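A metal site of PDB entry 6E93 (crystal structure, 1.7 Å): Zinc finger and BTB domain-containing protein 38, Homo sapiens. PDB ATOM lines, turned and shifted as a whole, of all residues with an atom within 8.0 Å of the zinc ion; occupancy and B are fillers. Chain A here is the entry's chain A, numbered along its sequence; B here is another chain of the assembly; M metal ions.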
ATOM      1  N   VAL A  62      25.467  -0.207 -21.022  1.00  0.00           N
ATOM      2  CA  VAL A  62      25.141  -0.788 -22.317  1.00  0.00           C
ATOM      3  C   VAL A  62      23.627  -0.907 -22.441  1.00  0.00           C
ATOM      4  O   VAL A  62      22.963  -1.391 -21.510  1.00  0.00           O
ATOM      5  CB  VAL A  62      25.792  -2.171 -22.482  1.00  0.00           C
ATOM      6  CG1 VAL A  62      25.396  -2.777 -23.835  1.00  0.00           C
ATOM      7  CG2 VAL A  62      27.303  -2.074 -22.323  1.00  0.00           C
ATOM      8  N   CYS A  63      23.097  -0.469 -23.575  1.00  0.00           N
ATOM      9  CA  CYS A  63      21.654  -0.507 -23.824  1.00  0.00           C
ATOM     10  C   CYS A  63      21.165  -1.939 -24.018  1.00  0.00           C
ATOM     11  O   CYS A  63      21.684  -2.680 -24.856  1.00  0.00           O
ATOM     12  CB  CYS A  63      21.328   0.329 -25.048  1.00  0.00           C
ATOM     13  SG  CYS A  63      19.594   0.312 -25.545  1.00  0.00           S
ATOM     14  N   GLN A  64      20.156  -2.326 -23.231  1.00  0.00           N
ATOM     15  CA  GLN A  64      19.610  -3.675 -23.309  1.00  0.00           C
ATOM     16  C   GLN A  64      18.818  -3.922 -24.579  1.00  0.00           C
ATOM     17  O   GLN A  64      18.440  -5.077 -24.829  1.00  0.00           O
ATOM     18  CB  GLN A  64      18.707  -3.933 -22.099  1.00  0.00           C
ATOM     19  CG  GLN A  64      17.516  -2.986 -22.020  1.00  0.00           C
ATOM     20  CD  GLN A  64      16.702  -3.180 -20.768  1.00  0.00           C
ATOM     21  OE1 GLN A  64      16.240  -4.290 -20.484  1.00  0.00           O
ATOM     22  NE2 GLN A  64      16.506  -2.112 -20.008  1.00  0.00           N
ATOM     23  N   TYR A  65      18.519  -2.890 -25.366  1.00  0.00           N
ATOM     24  CA  TYR A  65      17.716  -3.032 -26.571  1.00  0.00           C
ATOM     25  C   TYR A  65      18.555  -3.052 -27.837  1.00  0.00           C
ATOM     26  O   TYR A  65      18.337  -3.896 -28.708  1.00  0.00           O
ATOM     27  CB  TYR A  65      16.664  -1.916 -26.665  1.00  0.00           C
ATOM     28  CG  TYR A  65      15.747  -1.848 -25.455  1.00  0.00           C
ATOM     29  CD1 TYR A  65      14.689  -2.724 -25.299  1.00  0.00           C
ATOM     30  CD2 TYR A  65      15.955  -0.894 -24.465  1.00  0.00           C
ATOM     31  CE1 TYR A  65      13.848  -2.666 -24.190  1.00  0.00           C
ATOM     32  CE2 TYR A  65      15.133  -0.825 -23.351  1.00  0.00           C
ATOM     33  CZ  TYR A  65      14.089  -1.703 -23.215  1.00  0.00           C
ATOM     34  OH  TYR A  65      13.276  -1.620 -22.105  1.00  0.00           O
ATOM     35  N   CYS A  66      19.535  -2.155 -27.963  1.00  0.00           N
ATOM     36  CA  CYS A  66      20.377  -2.113 -29.156  1.00  0.00           C
ATOM     37  C   CYS A  66      21.856  -2.341 -28.884  1.00  0.00           C
ATOM     38  O   CYS A  66      22.621  -2.455 -29.850  1.00  0.00           O
ATOM     39  CB  CYS A  66      20.201  -0.780 -29.894  1.00  0.00           C
ATOM     40  SG  CYS A  66      20.995   0.615 -29.054  1.00  0.00           S
ATOM     41  N   ASN A  67      22.287  -2.411 -27.620  1.00  0.00           N
ATOM     42  CA  ASN A  67      23.646  -2.766 -27.202  1.00  0.00           C
ATOM     43  C   ASN A  67      24.636  -1.621 -27.373  1.00  0.00           C
ATOM     44  O   ASN A  67      25.846  -1.844 -27.215  1.00  0.00           O
ATOM     45  CB  ASN A  67      24.174  -4.010 -27.950  1.00  0.00           C
ATOM     46  CG  ASN A  67      25.224  -4.763 -27.146  1.00  0.00           C
ATOM     47  OD1 ASN A  67      24.963  -5.201 -26.028  1.00  0.00           O
ATOM     48  ND2 ASN A  67      26.409  -4.949 -27.740  1.00  0.00           N
ATOM     49  N   LYS A  68      24.187  -0.406 -27.694  1.00  0.00           N
ATOM     50  CA  LYS A  68      25.102   0.729 -27.697  1.00  0.00           C
ATOM     51  C   LYS A  68      25.552   1.027 -26.280  1.00  0.00           C
ATOM     52  O   LYS A  68      24.787   0.879 -25.325  1.00  0.00           O
ATOM     53  CB  LYS A  68      24.449   1.971 -28.308  1.00  0.00           C
ATOM     54  CG  LYS A  68      25.389   3.175 -28.317  1.00  0.00           C
ATOM     55  CD  LYS A  68      24.905   4.303 -29.231  1.00  0.00           C
ATOM     56  CE  LYS A  68      25.871   5.489 -29.201  1.00  0.00           C
ATOM     57  NZ  LYS A  68      25.392   6.606 -30.076  1.00  0.00           N
ATOM     58  N   ALA A  69      26.816   1.448 -26.127  1.00  0.00           N
ATOM     59  CA  ALA A  69      27.434   1.671 -24.832  1.00  0.00           C
ATOM     60  C   ALA A  69      27.634   3.170 -24.586  1.00  0.00           C
ATOM     61  O   ALA A  69      27.841   3.944 -25.516  1.00  0.00           O
ATOM     62  CB  ALA A  69      28.776   0.955 -24.724  1.00  0.00           C
ATOM     63  N   PHE A  70      27.556   3.556 -23.305  1.00  0.00           N
ATOM     64  CA  PHE A  70      27.633   4.950 -22.916  1.00  0.00           C
ATOM     65  C   PHE A  70      28.547   5.110 -21.714  1.00  0.00           C
ATOM     66  O   PHE A  70      28.734   4.177 -20.928  1.00  0.00           O
ATOM     67  CB  PHE A  70      26.235   5.502 -22.587  1.00  0.00           C
ATOM     68  CG  PHE A  70      25.275   5.386 -23.716  1.00  0.00           C
ATOM     69  CD1 PHE A  70      24.531   4.227 -23.893  1.00  0.00           C
ATOM     70  CD2 PHE A  70      25.126   6.416 -24.625  1.00  0.00           C
ATOM     71  CE1 PHE A  70      23.633   4.110 -24.952  1.00  0.00           C
ATOM     72  CE2 PHE A  70      24.238   6.316 -25.699  1.00  0.00           C
ATOM     73  CZ  PHE A  70      23.492   5.163 -25.863  1.00  0.00           C
ATOM     74  N   LEU A  76      22.907   6.576 -20.655  1.00  0.00           N
ATOM     75  CA  LEU A  76      22.223   5.360 -21.065  1.00  0.00           C
ATOM     76  C   LEU A  76      20.717   5.466 -20.851  1.00  0.00           C
ATOM     77  O   LEU A  76      19.929   5.135 -21.746  1.00  0.00           O
ATOM     78  CB  LEU A  76      22.795   4.171 -20.288  1.00  0.00           C
ATOM     79  CG  LEU A  76      21.906   2.936 -20.462  1.00  0.00           C
ATOM     80  CD1 LEU A  76      21.898   2.535 -21.906  1.00  0.00           C
ATOM     81  CD2 LEU A  76      22.387   1.797 -19.584  1.00  0.00           C
ATOM     82  N   HIS A  79      18.913   7.569 -23.246  1.00  0.00           N
ATOM     83  CA  HIS A  79      18.872   6.893 -24.539  1.00  0.00           C
ATOM     84  C   HIS A  79      17.792   5.829 -24.574  1.00  0.00           C
ATOM     85  O   HIS A  79      17.093   5.686 -25.588  1.00  0.00           O
ATOM     86  CB  HIS A  79      20.239   6.279 -24.818  1.00  0.00           C
ATOM     87  CG  HIS A  79      20.205   5.256 -25.907  1.00  0.00           C
ATOM     88  ND1 HIS A  79      20.336   5.580 -27.235  1.00  0.00           N
ATOM     89  CD2 HIS A  79      20.057   3.906 -25.855  1.00  0.00           C
ATOM     90  CE1 HIS A  79      20.257   4.484 -27.972  1.00  0.00           C
ATOM     91  NE2 HIS A  79      20.085   3.444 -27.156  1.00  0.00           N
ATOM     92  N   GLU A  80      17.635   5.051 -23.502  1.00  0.00           N
ATOM     93  CA  GLU A  80      16.694   3.938 -23.548  1.00  0.00           C
ATOM     94  C   GLU A  80      15.252   4.408 -23.694  1.00  0.00           C
ATOM     95  O   GLU A  80      14.410   3.648 -24.185  1.00  0.00           O
ATOM     96  CB  GLU A  80      16.843   3.043 -22.321  1.00  0.00           C
ATOM     97  CG  GLU A  80      18.151   2.256 -22.345  1.00  0.00           C
ATOM     98  CD  GLU A  80      18.145   1.039 -21.420  1.00  0.00           C
ATOM     99  OE1 GLU A  80      17.178   0.856 -20.658  1.00  0.00           O
ATOM    100  OE2 GLU A  80      19.129   0.262 -21.467  1.00  0.00           O
ATOM    101  N   ARG A  81      14.948   5.642 -23.284  1.00  0.00           N
ATOM    102  CA  ARG A  81      13.613   6.200 -23.528  1.00  0.00           C
ATOM    103  C   ARG A  81      13.191   6.079 -24.990  1.00  0.00           C
ATOM    104  O   ARG A  81      11.998   5.946 -25.284  1.00  0.00           O
ATOM    105  CB  ARG A  81      13.577   7.662 -23.108  1.00  0.00           C
ATOM    106  CG  ARG A  81      13.834   7.868 -21.627  1.00  0.00           C
ATOM    107  CD  ARG A  81      13.923   9.351 -21.313  1.00  0.00           C
ATOM    108  NE  ARG A  81      14.324   9.588 -19.932  1.00  0.00           N
ATOM    109  CZ  ARG A  81      14.700  10.776 -19.481  1.00  0.00           C
ATOM    110  NH1 ARG A  81      14.718  11.825 -20.301  1.00  0.00           N
ATOM    111  NH2 ARG A  81      15.066  10.928 -18.216  1.00  0.00           N
ATOM    112  N   ILE A  82      14.152   6.149 -25.906  1.00  0.00           N
ATOM    113  CA  ILE A  82      13.837   6.021 -27.327  1.00  0.00           C
ATOM    114  C   ILE A  82      13.163   4.683 -27.574  1.00  0.00           C
ATOM    115  O   ILE A  82      12.187   4.600 -28.336  1.00  0.00           O
ATOM    116  CB  ILE A  82      15.116   6.161 -28.174  1.00  0.00           C
ATOM    117  CG1 ILE A  82      15.735   7.546 -28.002  1.00  0.00           C
ATOM    118  CG2 ILE A  82      14.845   5.874 -29.641  1.00  0.00           C
ATOM    119  CD1 ILE A  82      17.167   7.648 -28.548  1.00  0.00           C
ATOM    120  N   HIS A  83      13.661   3.623 -26.943  1.00  0.00           N
ATOM    121  CA  HIS A  83      13.137   2.279 -27.165  1.00  0.00           C
ATOM    122  C   HIS A  83      11.840   2.047 -26.404  1.00  0.00           C
ATOM    123  O   HIS A  83      10.906   1.432 -26.931  1.00  0.00           O
ATOM    124  CB  HIS A  83      14.163   1.225 -26.737  1.00  0.00           C
ATOM    125  CG  HIS A  83      15.460   1.309 -27.463  1.00  0.00           C
ATOM    126  ND1 HIS A  83      15.578   1.024 -28.812  1.00  0.00           N
ATOM    127  CD2 HIS A  83      16.707   1.598 -27.027  1.00  0.00           C
ATOM    128  CE1 HIS A  83      16.846   1.158 -29.165  1.00  0.00           C
ATOM    129  NE2 HIS A  83      17.558   1.500 -28.106  1.00  0.00           N
ATOM    130  N1  5CM B   6      23.086  13.557 -26.737  1.00  0.00           N
ATOM    131  C2  5CM B   6      23.443  14.909 -26.828  1.00  0.00           C
ATOM    132  N3  5CM B   6      22.535  15.851 -26.528  1.00  0.00           N
ATOM    133  C4  5CM B   6      21.301  15.556 -26.150  1.00  0.00           C
ATOM    134  C5  5CM B   6      20.885  14.183 -26.052  1.00  0.00           C
ATOM    135  C5A 5CM B   6      19.480  13.805 -25.625  1.00  0.00           C
ATOM    136  C6  5CM B   6      21.826  13.215 -26.356  1.00  0.00           C
ATOM    137  O2  5CM B   6      24.587  15.233 -27.175  1.00  0.00           O
ATOM    138  N4  5CM B   6      20.474  16.542 -25.879  1.00  0.00           N
ATOM    139  C1' 5CM B   6      24.102  12.543 -27.027  1.00  0.00           C
ATOM    140  C2' 5CM B   6      23.995  11.253 -26.191  1.00  0.00           C
ATOM    141  C3' 5CM B   6      25.064  10.423 -26.912  1.00  0.00           C
ATOM    142  C4' 5CM B   6      24.856  10.862 -28.368  1.00  0.00           C
ATOM    143  O4' 5CM B   6      24.064  12.068 -28.350  1.00  0.00           O
ATOM    144  O3' 5CM B   6      26.315  10.791 -26.355  1.00  0.00           O
ATOM    145  C5' 5CM B   6      24.124   9.832 -29.199  1.00  0.00           C
ATOM    146  O5' 5CM B   6      23.040   9.301 -28.426  1.00  0.00           O
ATOM    147  P   5CM B   6      21.976   8.338 -29.124  1.00  0.00           P
ATOM    148  OP1 5CM B   6      22.633   7.138 -29.674  1.00  0.00           O
ATOM    149  OP2 5CM B   6      20.921   8.067 -28.115  1.00  0.00           O
HETATM  150 ZN    ZN M   1      19.600   1.394 -27.540  1.00  0.00          ZN
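The side-chain sulfur of Cys 66 sits close to the backbone NH of Lys 68. The backbone carbonyl oxygen of Lys 68 lies within hydrogen-bond range of the backbone NH of Cys 63, at 2.8 Å. N of Tyr 65 sits close to SG of Cys 63, 3.4 Å away. A ring nitrogen (ND1) of His 79 sits at hydrogen-bond distance from OP2 of 5CM 6 of chain B (2.7 Å).
Of the 16 residues printed, 4 come within 4 Å of the zinc ion. The nearest printed residue that does not touch the zinc ion is Tyr 65 (4.5 Å).
A ring nitrogen (NE2) of His 83 binds the zinc ion, 2.1 Å away. NE2 of His 79 is bound to the zinc ion (2.1 Å). SG of Cys 66 binds the zinc ion (2.2 Å). The zinc ion is bound by the side-chain sulfur (SG) of Cys 63, 2.3 Å away. The zinc ion has four donor atoms within binding distance.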
